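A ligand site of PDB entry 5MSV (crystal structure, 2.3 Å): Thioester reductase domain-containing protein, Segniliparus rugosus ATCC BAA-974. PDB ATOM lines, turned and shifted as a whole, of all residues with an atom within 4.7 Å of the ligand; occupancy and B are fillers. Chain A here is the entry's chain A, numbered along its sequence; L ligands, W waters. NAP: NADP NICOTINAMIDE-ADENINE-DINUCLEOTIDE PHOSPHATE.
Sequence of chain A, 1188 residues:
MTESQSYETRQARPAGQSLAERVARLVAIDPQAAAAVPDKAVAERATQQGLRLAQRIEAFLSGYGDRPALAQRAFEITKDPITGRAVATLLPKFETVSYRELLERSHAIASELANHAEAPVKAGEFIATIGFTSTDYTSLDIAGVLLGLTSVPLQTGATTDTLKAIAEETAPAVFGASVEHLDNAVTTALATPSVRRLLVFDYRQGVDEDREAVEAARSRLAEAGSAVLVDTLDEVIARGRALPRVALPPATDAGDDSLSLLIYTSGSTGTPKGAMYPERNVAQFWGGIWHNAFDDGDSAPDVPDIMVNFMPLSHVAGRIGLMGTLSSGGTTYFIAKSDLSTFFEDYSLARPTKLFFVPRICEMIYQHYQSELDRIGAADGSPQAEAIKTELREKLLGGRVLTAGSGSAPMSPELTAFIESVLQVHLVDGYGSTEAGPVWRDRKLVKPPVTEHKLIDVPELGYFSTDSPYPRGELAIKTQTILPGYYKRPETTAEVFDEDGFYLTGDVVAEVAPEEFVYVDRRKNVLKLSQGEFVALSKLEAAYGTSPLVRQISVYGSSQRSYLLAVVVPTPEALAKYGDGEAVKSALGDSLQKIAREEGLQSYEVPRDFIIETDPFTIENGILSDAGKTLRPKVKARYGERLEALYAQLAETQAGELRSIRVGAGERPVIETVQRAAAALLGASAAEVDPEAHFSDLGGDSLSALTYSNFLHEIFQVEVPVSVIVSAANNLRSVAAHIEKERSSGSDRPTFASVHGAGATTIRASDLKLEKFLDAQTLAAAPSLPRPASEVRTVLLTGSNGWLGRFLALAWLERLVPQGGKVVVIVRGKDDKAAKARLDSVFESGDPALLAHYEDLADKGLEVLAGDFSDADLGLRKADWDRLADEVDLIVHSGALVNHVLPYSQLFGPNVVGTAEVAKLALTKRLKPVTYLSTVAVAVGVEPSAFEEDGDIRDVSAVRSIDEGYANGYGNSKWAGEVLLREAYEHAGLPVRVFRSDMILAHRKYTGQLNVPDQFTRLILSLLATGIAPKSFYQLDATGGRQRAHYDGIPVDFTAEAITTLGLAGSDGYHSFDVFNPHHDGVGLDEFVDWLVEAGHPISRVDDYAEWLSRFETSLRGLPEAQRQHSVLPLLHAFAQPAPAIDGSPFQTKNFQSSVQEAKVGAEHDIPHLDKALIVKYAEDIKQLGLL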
ATOM      1  N   GLY A 799      -0.639  -3.561  12.289  1.00  0.00           N
ATOM      2  CA  GLY A 799      -0.815  -2.591  13.371  1.00  0.00           C
ATOM      3  C   GLY A 799      -0.487  -1.136  13.051  1.00  0.00           C
ATOM      4  O   GLY A 799      -0.206  -0.350  13.969  1.00  0.00           O
ATOM      5  N   SER A 800      -0.588  -0.764  11.772  1.00  0.00           N
ATOM      6  CA  SER A 800      -0.177   0.567  11.304  1.00  0.00           C
ATOM      7  C   SER A 800      -0.959   1.757  11.875  1.00  0.00           C
ATOM      8  O   SER A 800      -0.412   2.855  11.961  1.00  0.00           O
ATOM      9  CB  SER A 800      -0.212   0.647   9.779  1.00  0.00           C
ATOM     10  OG  SER A 800      -1.535   0.483   9.276  1.00  0.00           O
ATOM     11  N   ASN A 801      -2.220   1.564  12.253  1.00  0.00           N
ATOM     12  CA  ASN A 801      -2.980   2.659  12.888  1.00  0.00           C
ATOM     13  C   ASN A 801      -2.782   2.725  14.408  1.00  0.00           C
ATOM     14  O   ASN A 801      -3.294   3.645  15.065  1.00  0.00           O
ATOM     15  CB  ASN A 801      -4.472   2.588  12.530  1.00  0.00           C
ATOM     16  CG  ASN A 801      -5.163   1.383  13.139  1.00  0.00           C
ATOM     17  OD1 ASN A 801      -4.794   0.242  12.855  1.00  0.00           O
ATOM     18  ND2 ASN A 801      -6.160   1.621  13.962  1.00  0.00           N
ATOM     19  N   GLY A 802      -2.059   1.753  14.954  1.00  0.00           N
ATOM     20  CA  GLY A 802      -1.648   1.771  16.347  1.00  0.00           C
ATOM     21  C   GLY A 802      -0.572   2.809  16.617  1.00  0.00           C
ATOM     22  O   GLY A 802      -0.118   3.520  15.715  1.00  0.00           O
ATOM     23  N   TRP A 803      -0.172   2.878  17.884  1.00  0.00           N
ATOM     24  CA  TRP A 803       0.767   3.897  18.322  1.00  0.00           C
ATOM     25  C   TRP A 803       2.154   3.757  17.687  1.00  0.00           C
ATOM     26  O   TRP A 803       2.636   4.679  17.048  1.00  0.00           O
ATOM     27  CB  TRP A 803       0.879   3.906  19.864  1.00  0.00           C
ATOM     28  CG  TRP A 803       1.983   4.769  20.340  1.00  0.00           C
ATOM     29  CD1 TRP A 803       3.036   4.405  21.114  1.00  0.00           C
ATOM     30  CD2 TRP A 803       2.174   6.164  20.039  1.00  0.00           C
ATOM     31  NE1 TRP A 803       3.853   5.475  21.341  1.00  0.00           N
ATOM     32  CE2 TRP A 803       3.353   6.570  20.686  1.00  0.00           C
ATOM     33  CE3 TRP A 803       1.440   7.106  19.301  1.00  0.00           C
ATOM     34  CZ2 TRP A 803       3.832   7.878  20.624  1.00  0.00           C
ATOM     35  CZ3 TRP A 803       1.926   8.408  19.236  1.00  0.00           C
ATOM     36  CH2 TRP A 803       3.112   8.778  19.881  1.00  0.00           C
ATOM     37  N   LEU A 804       2.800   2.618  17.879  1.00  0.00           N
ATOM     38  CA  LEU A 804       4.128   2.408  17.309  1.00  0.00           C
ATOM     39  C   LEU A 804       4.050   2.189  15.794  1.00  0.00           C
ATOM     40  O   LEU A 804       4.876   2.728  15.050  1.00  0.00           O
ATOM     41  CB  LEU A 804       4.823   1.199  17.969  1.00  0.00           C
ATOM     42  CG  LEU A 804       6.201   0.794  17.451  1.00  0.00           C
ATOM     43  CD1 LEU A 804       7.186   1.958  17.440  1.00  0.00           C
ATOM     44  CD2 LEU A 804       6.744  -0.348  18.284  1.00  0.00           C
ATOM     45  N   GLY A 805       3.068   1.402  15.356  1.00  0.00           N
ATOM     46  CA  GLY A 805       2.930   1.045  13.958  1.00  0.00           C
ATOM     47  C   GLY A 805       2.842   2.188  12.962  1.00  0.00           C
ATOM     48  O   GLY A 805       3.350   2.069  11.844  1.00  0.00           O
ATOM     49  N   ARG A 828      -8.051  -3.094  10.394  1.00  0.00           N
ATOM     50  CA  ARG A 828      -9.417  -3.524  10.629  1.00  0.00           C
ATOM     51  C   ARG A 828     -10.397  -2.449  10.165  1.00  0.00           C
ATOM     52  O   ARG A 828     -10.200  -1.242  10.413  1.00  0.00           O
ATOM     53  CB  ARG A 828      -9.669  -3.877  12.102  1.00  0.00           C
ATOM     54  CG  ARG A 828      -8.947  -5.144  12.549  1.00  0.00           C
ATOM     55  CD  ARG A 828      -9.532  -5.737  13.819  1.00  0.00           C
ATOM     56  NE  ARG A 828      -9.263  -4.918  15.001  1.00  0.00           N
ATOM     57  CZ  ARG A 828      -9.631  -5.235  16.248  1.00  0.00           C
ATOM     58  NH1 ARG A 828     -10.303  -6.357  16.511  1.00  0.00           N
ATOM     59  NH2 ARG A 828      -9.327  -4.409  17.243  1.00  0.00           N
ATOM     60  N   ARG A 838      -9.555   5.153   8.688  1.00  0.00           N
ATOM     61  CA  ARG A 838      -9.059   4.946  10.054  1.00  0.00           C
ATOM     62  C   ARG A 838      -7.559   5.232  10.158  1.00  0.00           C
ATOM     63  O   ARG A 838      -7.131   5.917  11.086  1.00  0.00           O
ATOM     64  CB  ARG A 838      -9.347   3.521  10.535  1.00  0.00           C
ATOM     65  CG  ARG A 838     -10.816   3.223  10.778  1.00  0.00           C
ATOM     66  CD  ARG A 838     -10.999   1.857  11.414  1.00  0.00           C
ATOM     67  NE  ARG A 838     -10.602   1.883  12.826  1.00  0.00           N
ATOM     68  CZ  ARG A 838      -9.793   1.015  13.430  1.00  0.00           C
ATOM     69  NH1 ARG A 838      -9.255  -0.043  12.813  1.00  0.00           N
ATOM     70  NH2 ARG A 838      -9.533   1.201  14.728  1.00  0.00           N
ATOM     71  N   GLY A 867      -8.649  -5.982   6.712  1.00  0.00           N
ATOM     72  CA  GLY A 867      -8.376  -7.359   7.091  1.00  0.00           C
ATOM     73  C   GLY A 867      -8.375  -7.554   8.585  1.00  0.00           C
ATOM     74  O   GLY A 867      -8.782  -6.691   9.346  1.00  0.00           O
ATOM     75  N   ASP A 868      -7.903  -8.725   8.992  1.00  0.00           N
ATOM     76  CA  ASP A 868      -7.924  -9.138  10.397  1.00  0.00           C
ATOM     77  C   ASP A 868      -6.965 -10.312  10.528  1.00  0.00           C
ATOM     78  O   ASP A 868      -7.255 -11.406  10.024  1.00  0.00           O
ATOM     79  CB  ASP A 868      -9.348  -9.533  10.806  1.00  0.00           C
ATOM     80  CG  ASP A 868      -9.490  -9.783  12.298  1.00  0.00           C
ATOM     81  OD1 ASP A 868      -8.650 -10.502  12.886  1.00  0.00           O
ATOM     82  OD2 ASP A 868     -10.453  -9.263  12.895  1.00  0.00           O
ATOM     83  N   PHE A 869      -5.840 -10.112  11.209  1.00  0.00           N
ATOM     84  CA  PHE A 869      -4.806 -11.160  11.274  1.00  0.00           C
ATOM     85  C   PHE A 869      -5.172 -12.364  12.154  1.00  0.00           C
ATOM     86  O   PHE A 869      -4.503 -13.379  12.100  1.00  0.00           O
ATOM     87  CB  PHE A 869      -3.391 -10.626  11.591  1.00  0.00           C
ATOM     88  CG  PHE A 869      -3.306  -9.741  12.799  1.00  0.00           C
ATOM     89  CD1 PHE A 869      -3.588 -10.218  14.063  1.00  0.00           C
ATOM     90  CD2 PHE A 869      -2.909  -8.431  12.671  1.00  0.00           C
ATOM     91  CE1 PHE A 869      -3.494  -9.394  15.176  1.00  0.00           C
ATOM     92  CE2 PHE A 869      -2.809  -7.600  13.780  1.00  0.00           C
ATOM     93  CZ  PHE A 869      -3.102  -8.084  15.039  1.00  0.00           C
ATOM     94  N   SER A 870      -6.249 -12.264  12.941  1.00  0.00           N
ATOM     95  CA  SER A 870      -6.758 -13.430  13.683  1.00  0.00           C
ATOM     96  C   SER A 870      -7.561 -14.409  12.793  1.00  0.00           C
ATOM     97  O   SER A 870      -7.804 -15.530  13.226  1.00  0.00           O
ATOM     98  CB  SER A 870      -7.606 -12.965  14.870  1.00  0.00           C
ATOM     99  OG  SER A 870      -8.886 -12.522  14.455  1.00  0.00           O
ATOM    100  N   SER A 894       3.627  -5.622  14.178  1.00  0.00           N
ATOM    101  CA  SER A 894       3.431  -4.734  15.336  1.00  0.00           C
ATOM    102  C   SER A 894       2.036  -4.801  15.942  1.00  0.00           C
ATOM    103  O   SER A 894       1.800  -4.265  17.018  1.00  0.00           O
ATOM    104  CB  SER A 894       3.731  -3.277  14.929  1.00  0.00           C
ATOM    105  OG  SER A 894       3.689  -2.421  16.053  1.00  0.00           O
ATOM    106  N   GLY A 895       1.117  -5.497  15.283  1.00  0.00           N
ATOM    107  CA  GLY A 895      -0.286  -5.453  15.675  1.00  0.00           C
ATOM    108  C   GLY A 895      -0.597  -6.455  16.767  1.00  0.00           C
ATOM    109  O   GLY A 895      -0.128  -7.582  16.725  1.00  0.00           O
ATOM    110  N   ALA A 896      -1.417  -6.035  17.716  1.00  0.00           N
ATOM    111  CA  ALA A 896      -1.833  -6.884  18.827  1.00  0.00           C
ATOM    112  C   ALA A 896      -2.956  -6.207  19.571  1.00  0.00           C
ATOM    113  O   ALA A 896      -3.134  -4.994  19.438  1.00  0.00           O
ATOM    114  CB  ALA A 896      -0.655  -7.145  19.765  1.00  0.00           C
ATOM    115  N   LEU A 897      -3.691  -6.974  20.367  1.00  0.00           N
ATOM    116  CA  LEU A 897      -4.615  -6.415  21.337  1.00  0.00           C
ATOM    117  C   LEU A 897      -3.813  -6.134  22.613  1.00  0.00           C
ATOM    118  O   LEU A 897      -3.451  -7.053  23.354  1.00  0.00           O
ATOM    119  CB  LEU A 897      -5.786  -7.354  21.601  1.00  0.00           C
ATOM    120  CG  LEU A 897      -6.832  -6.923  22.643  1.00  0.00           C
ATOM    121  CD1 LEU A 897      -7.223  -5.467  22.532  1.00  0.00           C
ATOM    122  CD2 LEU A 897      -8.073  -7.804  22.511  1.00  0.00           C
ATOM    123  N   VAL A 898      -3.511  -4.862  22.828  1.00  0.00           N
ATOM    124  CA  VAL A 898      -2.670  -4.410  23.939  1.00  0.00           C
ATOM    125  C   VAL A 898      -3.593  -3.959  25.044  1.00  0.00           C
ATOM    126  O   VAL A 898      -4.159  -2.868  24.982  1.00  0.00           O
ATOM    127  CB  VAL A 898      -1.745  -3.267  23.507  1.00  0.00           C
ATOM    128  CG1 VAL A 898      -0.812  -2.854  24.658  1.00  0.00           C
ATOM    129  CG2 VAL A 898      -0.943  -3.672  22.285  1.00  0.00           C
ATOM    130  N   PRO A 910      -6.249 -12.684  18.957  1.00  0.00           N
ATOM    131  CA  PRO A 910      -5.449 -11.662  18.280  1.00  0.00           C
ATOM    132  C   PRO A 910      -3.945 -11.850  18.400  1.00  0.00           C
ATOM    133  O   PRO A 910      -3.231 -11.645  17.405  1.00  0.00           O
ATOM    134  CB  PRO A 910      -5.887 -10.344  18.926  1.00  0.00           C
ATOM    135  CG  PRO A 910      -6.651 -10.717  20.150  1.00  0.00           C
ATOM    136  CD  PRO A 910      -7.164 -12.102  19.955  1.00  0.00           C
ATOM    137  N   LEU A 933       7.037  -7.494  17.430  1.00  0.00           N
ATOM    138  CA  LEU A 933       6.992  -6.663  18.629  1.00  0.00           C
ATOM    139  C   LEU A 933       6.518  -7.475  19.820  1.00  0.00           C
ATOM    140  O   LEU A 933       5.517  -8.183  19.742  1.00  0.00           O
ATOM    141  CB  LEU A 933       6.089  -5.447  18.426  1.00  0.00           C
ATOM    142  CG  LEU A 933       6.764  -4.190  17.858  1.00  0.00           C
ATOM    143  CD1 LEU A 933       7.715  -3.597  18.905  1.00  0.00           C
ATOM    144  CD2 LEU A 933       7.485  -4.452  16.548  1.00  0.00           C
ATOM    145  N   SER A 934       7.275  -7.388  20.913  1.00  0.00           N
ATOM    146  CA  SER A 934       6.948  -8.044  22.169  1.00  0.00           C
ATOM    147  C   SER A 934       7.017  -6.994  23.271  1.00  0.00           C
ATOM    148  O   SER A 934       6.860  -5.807  22.998  1.00  0.00           O
ATOM    149  CB  SER A 934       7.900  -9.235  22.411  1.00  0.00           C
ATOM    150  OG  SER A 934       7.486  -9.991  23.538  1.00  0.00           O
ATOM    151  N   THR A 935       7.278  -7.405  24.513  1.00  0.00           N
ATOM    152  CA  THR A 935       7.056  -6.533  25.653  1.00  0.00           C
ATOM    153  C   THR A 935       7.870  -6.977  26.862  1.00  0.00           C
ATOM    154  O   THR A 935       8.126  -8.172  27.039  1.00  0.00           O
ATOM    155  CB  THR A 935       5.556  -6.493  26.023  1.00  0.00           C
ATOM    156  OG1 THR A 935       5.362  -5.738  27.223  1.00  0.00           O
ATOM    157  CG2 THR A 935       4.989  -7.897  26.239  1.00  0.00           C
ATOM    158  N   TYR A 970      -1.847 -10.307  28.974  1.00  0.00           N
ATOM    159  CA  TYR A 970      -1.089  -9.621  27.945  1.00  0.00           C
ATOM    160  C   TYR A 970       0.332 -10.189  27.846  1.00  0.00           C
ATOM    161  O   TYR A 970       0.771 -10.570  26.764  1.00  0.00           O
ATOM    162  CB  TYR A 970      -1.070  -8.108  28.201  1.00  0.00           C
ATOM    163  CG  TYR A 970      -0.182  -7.335  27.263  1.00  0.00           C
ATOM    164  CD1 TYR A 970      -0.445  -7.299  25.881  1.00  0.00           C
ATOM    165  CD2 TYR A 970       0.946  -6.662  27.736  1.00  0.00           C
ATOM    166  CE1 TYR A 970       0.390  -6.610  25.016  1.00  0.00           C
ATOM    167  CE2 TYR A 970       1.768  -5.959  26.878  1.00  0.00           C
ATOM    168  CZ  TYR A 970       1.499  -5.936  25.513  1.00  0.00           C
ATOM    169  OH  TYR A 970       2.349  -5.252  24.686  1.00  0.00           O
ATOM    170  N   LYS A 974       1.898 -12.349  24.512  1.00  0.00           N
ATOM    171  CA  LYS A 974       3.070 -11.906  23.749  1.00  0.00           C
ATOM    172  C   LYS A 974       4.229 -12.915  23.816  1.00  0.00           C
ATOM    173  O   LYS A 974       4.946 -13.120  22.822  1.00  0.00           O
ATOM    174  CB  LYS A 974       3.537 -10.532  24.232  1.00  0.00           C
ATOM    175  CG  LYS A 974       2.497  -9.418  24.049  1.00  0.00           C
ATOM    176  CD  LYS A 974       2.047  -9.206  22.607  1.00  0.00           C
ATOM    177  CE  LYS A 974       3.209  -8.864  21.680  1.00  0.00           C
ATOM    178  NZ  LYS A 974       2.770  -8.456  20.324  1.00  0.00           N
ATOM    179  N   SER A 997       9.419  -4.197  23.952  1.00  0.00           N
ATOM    180  CA  SER A 997       9.320  -2.775  24.299  1.00  0.00           C
ATOM    181  C   SER A 997       9.030  -2.549  25.769  1.00  0.00           C
ATOM    182  O   SER A 997       8.351  -3.335  26.414  1.00  0.00           O
ATOM    183  CB  SER A 997       8.244  -2.096  23.448  1.00  0.00           C
ATOM    184  OG  SER A 997       6.937  -2.510  23.845  1.00  0.00           O
ATOM    185  N   ASN A1011       0.729   8.213  22.882  1.00  0.00           N
ATOM    186  CA  ASN A1011      -0.125   7.045  23.024  1.00  0.00           C
ATOM    187  C   ASN A1011      -1.174   7.356  24.075  1.00  0.00           C
ATOM    188  O   ASN A1011      -0.930   7.205  25.276  1.00  0.00           O
ATOM    189  CB  ASN A1011       0.703   5.814  23.416  1.00  0.00           C
ATOM    190  CG  ASN A1011      -0.057   4.514  23.238  1.00  0.00           C
ATOM    191  OD1 ASN A1011      -1.253   4.519  22.917  1.00  0.00           O
ATOM    192  ND2 ASN A1011       0.617   3.391  23.448  1.00  0.00           N
HETATM  193  PA  NAP L   1      -1.708  -0.298  19.870  1.00  0.00           P
HETATM  194  O1A NAP L   1      -1.482   1.168  19.695  1.00  0.00           O
HETATM  195  O2A NAP L   1      -2.767  -0.807  20.803  1.00  0.00           O
HETATM  196  O5B NAP L   1      -1.969  -0.860  18.407  1.00  0.00           O
HETATM  197  C5B NAP L   1      -2.418  -2.180  18.169  1.00  0.00           C
HETATM  198  C4B NAP L   1      -2.591  -2.331  16.662  1.00  0.00           C
HETATM  199  O4B NAP L   1      -2.899  -3.687  16.315  1.00  0.00           O
HETATM  200  C3B NAP L   1      -3.788  -1.512  16.182  1.00  0.00           C
HETATM  201  O3B NAP L   1      -3.542  -1.039  14.859  1.00  0.00           O
HETATM  202  C2B NAP L   1      -4.904  -2.511  16.170  1.00  0.00           C
HETATM  203  O2B NAP L   1      -6.007  -2.143  15.356  1.00  0.00           O
HETATM  204  C1B NAP L   1      -4.139  -3.708  15.610  1.00  0.00           C
HETATM  205  N9A NAP L   1      -4.901  -4.957  15.795  1.00  0.00           N
HETATM  206  C8A NAP L   1      -5.342  -5.493  16.949  1.00  0.00           C
HETATM  207  N7A NAP L   1      -6.033  -6.638  16.695  1.00  0.00           N
HETATM  208  C5A NAP L   1      -6.038  -6.817  15.380  1.00  0.00           C
HETATM  209  C6A NAP L   1      -6.577  -7.831  14.460  1.00  0.00           C
HETATM  210  N6A NAP L   1      -7.266  -8.879  14.952  1.00  0.00           N
HETATM  211  N1A NAP L   1      -6.362  -7.670  13.140  1.00  0.00           N
HETATM  212  C2A NAP L   1      -5.685  -6.602  12.642  1.00  0.00           C
HETATM  213  N3A NAP L   1      -5.165  -5.637  13.424  1.00  0.00           N
HETATM  214  C4A NAP L   1      -5.304  -5.702  14.774  1.00  0.00           C
HETATM  215  O3  NAP L   1      -0.345  -1.066  20.255  1.00  0.00           O
HETATM  216  PN  NAP L   1       1.108  -0.365  20.326  1.00  0.00           P
HETATM  217  O1N NAP L   1       1.181   0.402  21.608  1.00  0.00           O
HETATM  218  O2N NAP L   1       1.358   0.313  18.999  1.00  0.00           O
HETATM  219  O5D NAP L   1       2.075  -1.638  20.470  1.00  0.00           O
HETATM  220  C5D NAP L   1       2.820  -2.152  19.372  1.00  0.00           C
HETATM  221  C4D NAP L   1       3.349  -3.553  19.653  1.00  0.00           C
HETATM  222  O4D NAP L   1       4.359  -3.497  20.686  1.00  0.00           O
HETATM  223  C3D NAP L   1       2.281  -4.522  20.139  1.00  0.00           C
HETATM  224  O3D NAP L   1       2.344  -5.762  19.438  1.00  0.00           O
HETATM  225  C2D NAP L   1       2.596  -4.708  21.604  1.00  0.00           C
HETATM  226  O2D NAP L   1       2.186  -5.973  22.114  1.00  0.00           O
HETATM  227  C1D NAP L   1       4.109  -4.524  21.647  1.00  0.00           C
HETATM  228  N1N NAP L   1       4.569  -4.083  22.959  1.00  0.00           N
HETATM  229  P2B NAP L   1      -7.414  -1.590  15.894  1.00  0.00           P
HETATM  230  O1X NAP L   1      -7.594  -2.092  17.308  1.00  0.00           O
HETATM  231  O2X NAP L   1      -7.328  -0.068  15.814  1.00  0.00           O
HETATM  232  O3X NAP L   1      -8.360  -2.196  14.881  1.00  0.00           O
HETATM  233  O   HOH W   1      -6.204  -2.217  12.411  1.00  0.00           O
HETATM  234  O   HOH W   2       2.712  -7.717  17.395  1.00  0.00           O
HETATM  235  O   HOH W   3      -3.244  -4.558  11.629  1.00  0.00           O
HETATM  236  O   HOH W   4      -7.926  -7.791  18.549  1.00  0.00           O
HETATM  237  O   HOH W   5      -6.796  -3.495  19.589  1.00  0.00           O
HETATM  238  O   HOH W   6     -10.981  -1.888  15.725  1.00  0.00           O
HETATM  239  O   HOH W   7      -3.273   0.695  23.090  1.00  0.00           O
HETATM  240  O   HOH W   8      -8.833 -10.118  17.022  1.00  0.00           O
HETATM  241  O   HOH W   9      -4.595  -2.713  21.275  1.00  0.00           O
HETATM  242  O   HOH W  10      -0.554   0.627  23.605  1.00  0.00           O
HETATM  243  O   HOH W  11       1.380  -0.683  16.483  1.00  0.00           O
HETATM  244  O   HOH W  12       3.806   1.201  22.421  1.00  0.00           O
HETATM  245  O   HOH W  13      -2.736   2.890  21.418  1.00  0.00           O
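The backbone NH (N) of Trp 803 lies within hydrogen-bond range of an oxygen (O1A) of the ligand, at 2.8 Å. An oxygen (O3B) of the ligand sits at hydrogen-bond distance from the side-chain amide oxygen (OD1) of Asn 801, 2.7 Å away. OH of Tyr 970 lies within hydrogen-bond range of O2D of the ligand, at 2.7 Å. The backbone NH of Ala 896 is in hydrogen-bond range of an oxygen (O4B) of the ligand (3.1 Å). An oxygen (O2X) of the ligand lies within salt-bridge range of the guanidinium group (NH2) of Arg 838, 2.8 Å away. An oxygen (O3X) of the ligand lies within salt-bridge range of the guanidinium group of Arg 828 (2.9 Å). A nitrogen (N1A) of the ligand is in hydrogen-bond range of the backbone NH (N) of Phe 869 (3.2 Å). N of Gly 802 lies within hydrogen-bond range of O3B of the ligand. The side-chain carboxylate of Asp 868 sits at hydrogen-bond distance from a nitrogen (N6A) of the ligand. O3D of the ligand is in hydrogen-bond range of O of Ser 894 (2.9 Å). OG of Ser 997 sits at hydrogen-bond distance from N1N of the ligand (3.0 Å). O3D of the ligand sits at hydrogen-bond distance from NZ of Lys 974 (2.9 Å). An oxygen (O2N) of the ligand is in hydrogen-bond range of the backbone NH of Leu 804 (2.9 Å).
The guanidinium group (NH1) of Arg 838 lies within hydrogen-bond range of the backbone carbonyl oxygen (O) of Arg 828. NZ of Lys 974 sits at hydrogen-bond distance from O of Leu 933 (2.8 Å). The side-chain carboxylate (OD1) of Asp 868 sits at hydrogen-bond distance from the side-chain hydroxyl (OG) of Ser 870, 2.6 Å away. N of Ser 997 is in hydrogen-bond range of O of Ser 934. The guanidinium group (NH2) of Arg 838 lies close to the side-chain amide nitrogen (ND2) of Asn 801 (3.5 Å).
N1N of the ligand lies close to O of Ser 934 (2.9 Å). Gly 799 touches the ligand (CA to O3B, 3.5 Å). Gly 895 touches the ligand (CA to O4B, 3.2 Å). CG2 of Val 898 touches O3 of the ligand, 3.4 Å away. Leu 933 touches the ligand (CB to O4D, 3.5 Å). ND2 of Asn 1011 touches O1N of the ligand, at 3.6 Å. Of the 26 residues printed, 19 come within 4 Å of the ligand.
Water W10 bridges an oxygen (O1N) of the ligand (2.7 Å) and the side-chain amide nitrogen of Asn 1011 (3.0 Å). Water W13 lies within hydrogen-bond range of the side-chain amide oxygen of Asn 1011 (2.7 Å) and an oxygen (O1A) of the ligand (2.7 Å). Water W6 bridges an oxygen (O3X) of the ligand (2.8 Å) and the guanidinium group (NH2) of Arg 828 (3.4 Å). Water W3 lies within hydrogen-bond range of N3A of the ligand and N of Gly 799. Water W2 lies within hydrogen-bond range of O3D of the ligand, O of Gly 895 and NZ of Lys 974. Water W4 bridges a nitrogen (N7A) of the ligand (2.9 Å) and the guanidinium group of Arg 828 (3.4 Å).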
